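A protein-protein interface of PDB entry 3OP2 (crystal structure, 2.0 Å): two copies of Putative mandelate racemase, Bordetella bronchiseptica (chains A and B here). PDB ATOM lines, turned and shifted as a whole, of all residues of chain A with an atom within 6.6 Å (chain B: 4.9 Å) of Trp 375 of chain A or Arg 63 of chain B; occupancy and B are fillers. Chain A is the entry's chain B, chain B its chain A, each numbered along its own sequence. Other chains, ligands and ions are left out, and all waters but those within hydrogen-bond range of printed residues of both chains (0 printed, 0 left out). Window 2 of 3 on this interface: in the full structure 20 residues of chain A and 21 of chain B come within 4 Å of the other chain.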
ATOM      1  N   HIS A  11      18.035 -16.906  26.809  1.00  0.00           N
ATOM      2  CA  HIS A  11      16.716 -16.752  26.200  1.00  0.00           C
ATOM      3  C   HIS A  11      16.612 -17.566  24.920  1.00  0.00           C
ATOM      4  O   HIS A  11      17.298 -17.284  23.937  1.00  0.00           O
ATOM      5  CB  HIS A  11      16.419 -15.284  25.909  1.00  0.00           C
ATOM      6  CG  HIS A  11      16.441 -14.413  27.123  1.00  0.00           C
ATOM      7  ND1 HIS A  11      17.567 -13.727  27.526  1.00  0.00           N
ATOM      8  CD2 HIS A  11      15.475 -14.117  28.026  1.00  0.00           C
ATOM      9  CE1 HIS A  11      17.294 -13.045  28.625  1.00  0.00           C
ATOM     10  NE2 HIS A  11      16.028 -13.259  28.945  1.00  0.00           N
ATOM     11  N   ALA A  12      15.745 -18.577  24.954  1.00  0.00           N
ATOM     12  CA  ALA A  12      15.510 -19.444  23.809  1.00  0.00           C
ATOM     13  C   ALA A  12      14.576 -18.750  22.818  1.00  0.00           C
ATOM     14  O   ALA A  12      13.460 -18.347  23.176  1.00  0.00           O
ATOM     15  CB  ALA A  12      14.937 -20.775  24.266  1.00  0.00           C
ATOM     16  N   LEU A  13      15.051 -18.583  21.587  1.00  0.00           N
ATOM     17  CA  LEU A  13      14.272 -17.937  20.540  1.00  0.00           C
ATOM     18  C   LEU A  13      14.153 -18.880  19.350  1.00  0.00           C
ATOM     19  O   LEU A  13      15.092 -19.610  19.036  1.00  0.00           O
ATOM     20  CB  LEU A  13      14.912 -16.606  20.124  1.00  0.00           C
ATOM     21  CG  LEU A  13      15.292 -15.578  21.208  1.00  0.00           C
ATOM     22  CD1 LEU A  13      15.909 -14.362  20.573  1.00  0.00           C
ATOM     23  CD2 LEU A  13      14.084 -15.161  22.050  1.00  0.00           C
ATOM     24  N   SER A  14      12.990 -18.885  18.705  1.00  0.00           N
ATOM     25  CA  SER A  14      12.765 -19.763  17.561  1.00  0.00           C
ATOM     26  C   SER A  14      11.752 -19.154  16.631  1.00  0.00           C
ATOM     27  O   SER A  14      10.614 -18.889  17.036  1.00  0.00           O
ATOM     28  CB  SER A  14      12.281 -21.143  18.008  1.00  0.00           C
ATOM     29  OG  SER A  14      12.169 -22.024  16.902  1.00  0.00           O
ATOM     30  N   GLN A  34      16.776 -20.751  15.022  1.00  0.00           N
ATOM     31  CA  GLN A  34      16.786 -20.717  16.478  1.00  0.00           C
ATOM     32  C   GLN A  34      18.089 -20.102  17.002  1.00  0.00           C
ATOM     33  O   GLN A  34      19.090 -20.023  16.274  1.00  0.00           O
ATOM     34  CB  GLN A  34      16.560 -22.122  17.066  1.00  0.00           C
ATOM     35  CG  GLN A  34      15.311 -22.844  16.521  1.00  0.00           C
ATOM     36  CD  GLN A  34      14.945 -24.107  17.285  1.00  0.00           C
ATOM     37  OE1 GLN A  34      15.808 -24.918  17.637  1.00  0.00           O
ATOM     38  NE2 GLN A  34      13.650 -24.295  17.522  1.00  0.00           N
ATOM     39  N   MET A  35      18.047 -19.638  18.248  1.00  0.00           N
ATOM     40  CA  MET A  35      19.240 -19.203  18.955  1.00  0.00           C
ATOM     41  C   MET A  35      18.956 -19.182  20.442  1.00  0.00           C
ATOM     42  O   MET A  35      17.800 -19.257  20.869  1.00  0.00           O
ATOM     43  CB  MET A  35      19.691 -17.806  18.500  1.00  0.00           C
ATOM     44  CG  MET A  35      18.826 -16.667  19.025  1.00  0.00           C
ATOM     45  SD  MET A  35      19.393 -14.912  18.399  1.00  0.00           S
ATOM     46  CE  MET A  35      20.923 -14.577  19.597  1.00  0.00           C
ATOM     47  N   ASP A  57      20.075 -28.253  20.397  1.00  0.00           N
ATOM     48  CA  ASP A  57      18.844 -28.252  21.187  1.00  0.00           C
ATOM     49  C   ASP A  57      18.791 -27.101  22.183  1.00  0.00           C
ATOM     50  O   ASP A  57      19.678 -26.958  23.021  1.00  0.00           O
ATOM     51  CB  ASP A  57      18.628 -29.562  21.926  1.00  0.00           C
ATOM     52  CG  ASP A  57      17.262 -29.625  22.576  1.00  0.00           C
ATOM     53  OD1 ASP A  57      16.284 -29.903  21.853  1.00  0.00           O
ATOM     54  OD2 ASP A  57      17.166 -29.378  23.798  1.00  0.00           O
ATOM     55  N   LEU A  58      17.733 -26.298  22.092  1.00  0.00           N
ATOM     56  CA  LEU A  58      17.640 -25.064  22.861  1.00  0.00           C
ATOM     57  C   LEU A  58      17.584 -25.304  24.361  1.00  0.00           C
ATOM     58  O   LEU A  58      18.174 -24.532  25.125  1.00  0.00           O
ATOM     59  CB  LEU A  58      16.450 -24.200  22.407  1.00  0.00           C
ATOM     60  CG  LEU A  58      16.589 -23.536  21.031  1.00  0.00           C
ATOM     61  CD1 LEU A  58      15.310 -22.824  20.653  1.00  0.00           C
ATOM     62  CD2 LEU A  58      17.767 -22.571  21.000  1.00  0.00           C
ATOM     63  N   ALA A  59      16.876 -26.359  24.767  1.00  0.00           N
ATOM     64  CA  ALA A  59      16.698 -26.687  26.180  1.00  0.00           C
ATOM     65  C   ALA A  59      17.996 -27.199  26.793  1.00  0.00           C
ATOM     66  O   ALA A  59      18.302 -26.870  27.932  1.00  0.00           O
ATOM     67  CB  ALA A  59      15.584 -27.701  26.364  1.00  0.00           C
ATOM     68  N   VAL A  60      18.740 -28.009  26.038  1.00  0.00           N
ATOM     69  CA  VAL A  60      20.097 -28.429  26.431  1.00  0.00           C
ATOM     70  C   VAL A  60      21.003 -27.204  26.673  1.00  0.00           C
ATOM     71  O   VAL A  60      21.614 -27.079  27.735  1.00  0.00           O
ATOM     72  CB  VAL A  60      20.719 -29.408  25.381  1.00  0.00           C
ATOM     73  CG1 VAL A  60      22.234 -29.583  25.595  1.00  0.00           C
ATOM     74  CG2 VAL A  60      20.012 -30.769  25.420  1.00  0.00           C
ATOM     75  N   LYS A  62      20.067 -23.933  27.108  1.00  0.00           N
ATOM     76  CA  LYS A  62      19.510 -23.121  28.177  1.00  0.00           C
ATOM     77  C   LYS A  62      19.902 -23.691  29.536  1.00  0.00           C
ATOM     78  O   LYS A  62      20.316 -22.943  30.429  1.00  0.00           O
ATOM     79  CB  LYS A  62      17.983 -23.051  28.057  1.00  0.00           C
ATOM     80  CG  LYS A  62      17.309 -22.124  29.049  1.00  0.00           C
ATOM     81  CD  LYS A  62      15.832 -21.922  28.702  1.00  0.00           C
ATOM     82  CE  LYS A  62      15.068 -21.235  29.838  1.00  0.00           C
ATOM     83  NZ  LYS A  62      15.464 -19.796  30.003  1.00  0.00           N
ATOM     84  N   HIS A 373       9.363 -13.774  20.344  1.00  0.00           N
ATOM     85  CA  HIS A 373       9.776 -15.019  19.705  1.00  0.00           C
ATOM     86  C   HIS A 373      10.328 -16.084  20.650  1.00  0.00           C
ATOM     87  O   HIS A 373      11.088 -16.955  20.227  1.00  0.00           O
ATOM     88  CB  HIS A 373      10.771 -14.716  18.585  1.00  0.00           C
ATOM     89  CG  HIS A 373      10.214 -13.828  17.519  1.00  0.00           C
ATOM     90  ND1 HIS A 373       9.421 -14.301  16.495  1.00  0.00           N
ATOM     91  CD2 HIS A 373      10.311 -12.491  17.330  1.00  0.00           C
ATOM     92  CE1 HIS A 373       9.073 -13.297  15.709  1.00  0.00           C
ATOM     93  NE2 HIS A 373       9.597 -12.188  16.197  1.00  0.00           N
ATOM     94  N   ALA A 374       9.934 -16.023  21.920  1.00  0.00           N
ATOM     95  CA  ALA A 374      10.308 -17.049  22.883  1.00  0.00           C
ATOM     96  C   ALA A 374       9.936 -18.428  22.357  1.00  0.00           C
ATOM     97  O   ALA A 374       8.869 -18.625  21.771  1.00  0.00           O
ATOM     98  CB  ALA A 374       9.655 -16.798  24.232  1.00  0.00           C
ATOM     99  N   TRP A 375      10.841 -19.375  22.556  1.00  0.00           N
ATOM    100  CA  TRP A 375      10.656 -20.744  22.115  1.00  0.00           C
ATOM    101  C   TRP A 375       9.526 -21.418  22.895  1.00  0.00           C
ATOM    102  O   TRP A 375       9.413 -21.247  24.111  1.00  0.00           O
ATOM    103  CB  TRP A 375      11.977 -21.475  22.312  1.00  0.00           C
ATOM    104  CG  TRP A 375      12.023 -22.906  21.939  1.00  0.00           C
ATOM    105  CD1 TRP A 375      11.754 -23.453  20.718  1.00  0.00           C
ATOM    106  CD2 TRP A 375      12.435 -23.983  22.781  1.00  0.00           C
ATOM    107  NE1 TRP A 375      11.954 -24.813  20.754  1.00  0.00           N
ATOM    108  CE2 TRP A 375      12.369 -25.165  22.011  1.00  0.00           C
ATOM    109  CE3 TRP A 375      12.840 -24.068  24.116  1.00  0.00           C
ATOM    110  CZ2 TRP A 375      12.691 -26.418  22.536  1.00  0.00           C
ATOM    111  CZ3 TRP A 375      13.159 -25.311  24.637  1.00  0.00           C
ATOM    112  CH2 TRP A 375      13.083 -26.471  23.848  1.00  0.00           C
ATOM    113  N   LYS A 376       8.689 -22.169  22.184  1.00  0.00           N
ATOM    114  CA  LYS A 376       7.570 -22.895  22.793  1.00  0.00           C
ATOM    115  C   LYS A 376       7.719 -24.416  22.662  1.00  0.00           C
ATOM    116  O   LYS A 376       6.929 -25.173  23.237  1.00  0.00           O
ATOM    117  CB  LYS A 376       6.246 -22.438  22.177  1.00  0.00           C
ATOM    118  CG  LYS A 376       5.889 -20.996  22.490  1.00  0.00           C
ATOM    119  CD  LYS A 376       4.740 -20.500  21.624  1.00  0.00           C
ATOM    120  CE  LYS A 376       4.208 -19.154  22.115  1.00  0.00           C
ATOM    121  NZ  LYS A 376       5.272 -18.104  22.192  1.00  0.00           N
ATOM    122  N   GLY A 377       8.727 -24.855  21.903  1.00  0.00           N
ATOM    123  CA  GLY A 377       9.004 -26.285  21.704  1.00  0.00           C
ATOM    124  C   GLY A 377       9.372 -26.697  20.283  1.00  0.00           C
ATOM    125  O   GLY A 377       9.576 -27.885  20.013  1.00  0.00           O
ATOM    126  N   GLU A 378       9.464 -25.713  19.384  1.00  0.00           N
ATOM    127  CA  GLU A 378       9.760 -25.927  17.957  1.00  0.00           C
ATOM    128  C   GLU A 378      11.147 -26.536  17.701  1.00  0.00           C
ATOM    129  O   GLU A 378      12.126 -26.144  18.344  1.00  0.00           O
ATOM    130  CB  GLU A 378       9.657 -24.609  17.172  1.00  0.00           C
ATOM    131  CG  GLU A 378       8.331 -23.862  17.273  1.00  0.00           C
ATOM    132  CD  GLU A 378       8.277 -22.919  18.463  1.00  0.00           C
ATOM    133  OE1 GLU A 378       8.025 -23.399  19.587  1.00  0.00           O
ATOM    134  OE2 GLU A 378       8.471 -21.701  18.271  1.00  0.00           O
ATOM    135  N   PRO A 379      11.228 -27.507  16.768  1.00  0.00           N
ATOM    136  CA  PRO A 379      12.503 -28.051  16.277  1.00  0.00           C
ATOM    137  C   PRO A 379      12.945 -27.452  14.925  1.00  0.00           C
ATOM    138  O   PRO A 379      12.184 -26.706  14.304  1.00  0.00           O
ATOM    139  CB  PRO A 379      12.204 -29.555  16.128  1.00  0.00           C
ATOM    140  CG  PRO A 379      10.707 -29.731  16.461  1.00  0.00           C
ATOM    141  CD  PRO A 379      10.101 -28.370  16.377  1.00  0.00           C
ATOM    142  N   ALA B  59      19.374 -33.197  33.663  1.00  0.00           N
ATOM    143  CA  ALA B  59      18.387 -32.577  32.784  1.00  0.00           C
ATOM    144  C   ALA B  59      18.914 -32.531  31.350  1.00  0.00           C
ATOM    145  O   ALA B  59      18.196 -32.874  30.416  1.00  0.00           O
ATOM    146  CB  ALA B  59      18.024 -31.188  33.275  1.00  0.00           C
ATOM    147  N   VAL B  60      20.180 -32.151  31.187  1.00  0.00           N
ATOM    148  CA  VAL B  60      20.823 -32.120  29.867  1.00  0.00           C
ATOM    149  C   VAL B  60      20.705 -33.506  29.215  1.00  0.00           C
ATOM    150  O   VAL B  60      20.279 -33.621  28.057  1.00  0.00           O
ATOM    151  CB  VAL B  60      22.321 -31.692  29.950  1.00  0.00           C
ATOM    152  CG1 VAL B  60      23.032 -31.897  28.611  1.00  0.00           C
ATOM    153  CG2 VAL B  60      22.452 -30.235  30.393  1.00  0.00           C
ATOM    154  N   LEU B  61      21.043 -34.551  29.978  1.00  0.00           N
ATOM    155  CA  LEU B  61      21.036 -35.904  29.444  1.00  0.00           C
ATOM    156  C   LEU B  61      19.643 -36.411  29.131  1.00  0.00           C
ATOM    157  O   LEU B  61      19.437 -37.013  28.073  1.00  0.00           O
ATOM    158  CB  LEU B  61      21.756 -36.886  30.370  1.00  0.00           C
ATOM    159  CG  LEU B  61      23.286 -36.874  30.396  1.00  0.00           C
ATOM    160  CD1 LEU B  61      23.754 -37.772  31.538  1.00  0.00           C
ATOM    161  CD2 LEU B  61      23.886 -37.334  29.066  1.00  0.00           C
ATOM    162  N   LYS B  62      18.698 -36.174  30.039  1.00  0.00           N
ATOM    163  CA  LYS B  62      17.305 -36.590  29.833  1.00  0.00           C
ATOM    164  C   LYS B  62      16.705 -35.954  28.565  1.00  0.00           C
ATOM    165  O   LYS B  62      16.057 -36.627  27.778  1.00  0.00           O
ATOM    166  CB  LYS B  62      16.455 -36.283  31.074  1.00  0.00           C
ATOM    167  CG  LYS B  62      15.026 -36.803  31.016  1.00  0.00           C
ATOM    168  CD  LYS B  62      14.275 -36.494  32.314  1.00  0.00           C
ATOM    169  CE  LYS B  62      12.813 -36.946  32.257  1.00  0.00           C
ATOM    170  NZ  LYS B  62      12.657 -38.433  32.161  1.00  0.00           N
ATOM    171  N   ARG B  63      16.956 -34.663  28.382  1.00  0.00           N
ATOM    172  CA  ARG B  63      16.479 -33.923  27.226  1.00  0.00           C
ATOM    173  C   ARG B  63      17.091 -34.483  25.934  1.00  0.00           C
ATOM    174  O   ARG B  63      16.370 -34.780  24.983  1.00  0.00           O
ATOM    175  CB  ARG B  63      16.796 -32.437  27.403  1.00  0.00           C
ATOM    176  CG  ARG B  63      16.504 -31.557  26.204  1.00  0.00           C
ATOM    177  CD  ARG B  63      15.010 -31.401  25.905  1.00  0.00           C
ATOM    178  NE  ARG B  63      14.832 -30.761  24.598  1.00  0.00           N
ATOM    179  CZ  ARG B  63      13.663 -30.504  24.020  1.00  0.00           C
ATOM    180  NH1 ARG B  63      12.523 -30.840  24.611  1.00  0.00           N
ATOM    181  NH2 ARG B  63      13.636 -29.922  22.830  1.00  0.00           N
ATOM    182  N   ALA B  64      18.412 -34.650  25.919  1.00  0.00           N
ATOM    183  CA  ALA B  64      19.103 -35.188  24.753  1.00  0.00           C
ATOM    184  C   ALA B  64      18.655 -36.614  24.409  1.00  0.00           C
ATOM    185  O   ALA B  64      18.419 -36.918  23.249  1.00  0.00           O
ATOM    186  CB  ALA B  64      20.599 -35.127  24.948  1.00  0.00           C
ATOM    187  N   ILE B  65      18.508 -37.474  25.411  1.00  0.00           N
ATOM    188  CA  ILE B  65      18.069 -38.850  25.158  1.00  0.00           C
ATOM    189  C   ILE B  65      16.604 -38.925  24.692  1.00  0.00           C
ATOM    190  O   ILE B  65      16.305 -39.527  23.649  1.00  0.00           O
ATOM    191  CB  ILE B  65      18.343 -39.768  26.372  1.00  0.00           C
ATOM    192  CG1 ILE B  65      19.859 -39.924  26.574  1.00  0.00           C
ATOM    193  CG2 ILE B  65      17.713 -41.131  26.182  1.00  0.00           C
ATOM    194  CD1 ILE B  65      20.257 -40.166  28.019  1.00  0.00           C
ATOM    195  N   GLU B  66      15.703 -38.291  25.441  1.00  0.00           N
ATOM    196  CA  GLU B  66      14.279 -38.400  25.153  1.00  0.00           C
ATOM    197  C   GLU B  66      13.818 -37.518  23.996  1.00  0.00           C
ATOM    198  O   GLU B  66      12.904 -37.894  23.261  1.00  0.00           O
ATOM    199  CB  GLU B  66      13.435 -38.083  26.387  1.00  0.00           C
ATOM    200  CG  GLU B  66      13.654 -39.029  27.557  1.00  0.00           C
ATOM    201  CD  GLU B  66      12.658 -38.818  28.689  1.00  0.00           C
ATOM    202  OE1 GLU B  66      12.015 -37.748  28.748  1.00  0.00           O
ATOM    203  OE2 GLU B  66      12.529 -39.732  29.527  1.00  0.00           O
ATOM    204  N   ASP B  67      14.425 -36.351  23.838  1.00  0.00           N
ATOM    205  CA  ASP B  67      13.842 -35.358  22.933  1.00  0.00           C
ATOM    206  C   ASP B  67      14.666 -35.061  21.700  1.00  0.00           C
ATOM    207  O   ASP B  67      14.181 -34.412  20.786  1.00  0.00           O
ATOM    208  CB  ASP B  67      13.513 -34.058  23.682  1.00  0.00           C
ATOM    209  CG  ASP B  67      12.472 -34.262  24.782  1.00  0.00           C
ATOM    210  OD1 ASP B  67      11.385 -34.789  24.480  1.00  0.00           O
ATOM    211  OD2 ASP B  67      12.733 -33.891  25.950  1.00  0.00           O
ATOM    212  N   VAL B  68      15.908 -35.534  21.675  1.00  0.00           N
ATOM    213  CA  VAL B  68      16.766 -35.334  20.518  1.00  0.00           C
ATOM    214  C   VAL B  68      17.040 -36.673  19.833  1.00  0.00           C
ATOM    215  O   VAL B  68      16.871 -36.800  18.625  1.00  0.00           O
ATOM    216  CB  VAL B  68      18.087 -34.612  20.891  1.00  0.00           C
ATOM    217  CG1 VAL B  68      18.948 -34.397  19.669  1.00  0.00           C
ATOM    218  CG2 VAL B  68      17.802 -33.272  21.560  1.00  0.00           C
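OD1 of Asp 57 of chain A lies within salt-bridge range of NH2 of Arg 63 of chain B, at 2.8 Å.
The side-chain carboxylate (OD2) of Asp 67 of chain B is in salt-bridge range of the guanidinium group (NH1) of Arg 63 of chain B, 3.3 Å away. O of Arg 63 of chain B is in hydrogen-bond range of N of Val 68 of chain B (3.4 Å). The backbone carbonyl oxygen (O) of Ala 12 of chain A sits at hydrogen-bond distance from the backbone NH (N) of Trp 375 of chain A. The side-chain carboxylate of Asp 57 of chain A lies within hydrogen-bond range of the backbone NH of Ala 59 of chain A (3.2 Å). The side-chain carboxylate (OD2) of Asp 57 of chain A is in hydrogen-bond range of the backbone NH (N) of Val 60 of chain A, at 3.1 Å. The indole nitrogen (NE1) of Trp 375 of chain A sits at hydrogen-bond distance from the backbone carbonyl oxygen (O) of Glu 378 of chain A.
Asp 57 of chain A touches Val 68 of chain B (OD1 to CG2, 3.7 Å). Ala 59 of chain A touches Arg 63 of chain B (CB to NE, 3.6 Å). Val 60 of chain A touches Val 60 of chain B. Arg 63 of chain B touches Val 60 of chain A. NH2 of Arg 63 of chain B touches CH2 of Trp 375 of chain A (3.6 Å).
Printed residues of chain B within 4 Å of Trp 375 of chain A: Arg 63. Arg 63 of chain B touches four residues of chain A. Of the printed residues of chain A, Val 60 of chain B touches Val 60 (3.9 Å). Of the printed residues of chain A, Val 68 of chain B touches Asp 57. Printed residues of chain B within 4 Å of Val 60 of chain A: Val 60 and Arg 63. Printed residues of chain B within 4 Å of Asp 57 of chain A: Arg 63 (2.8 Å) and Val 68 (3.7 Å). Printed residues of chain B within 4 Å of Ala 59 of chain A: Arg 63. Lys 376 of chain A touches none of the printed residues of chain B. Ala 59 of chain B touches none of the printed residues of chain A. The nearest residue of chain A that does not touch Arg 63 of chain B is Gly 377 of chain A (5.3 Å). The nearest printed residue of chain A that does not touch Val 68 of chain B is Val 60 of chain A (5.1 Å).
Printed residues of chain B that touch a printed residue of chain A: Val 60, Arg 63 and Val 68. Hydrophobic or aromatic side chains of chain A within 4 Å of the printed part of chain B: Ala 59, Val 60 and Trp 375.
Val 60 of chain A touches its own counterpart, Val 60 of chain B. 3 positions are printed for both chains. Of the 6 pairs that touch across the chains among the printed residues, 1 has its exchanged pair printed and touching as well.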
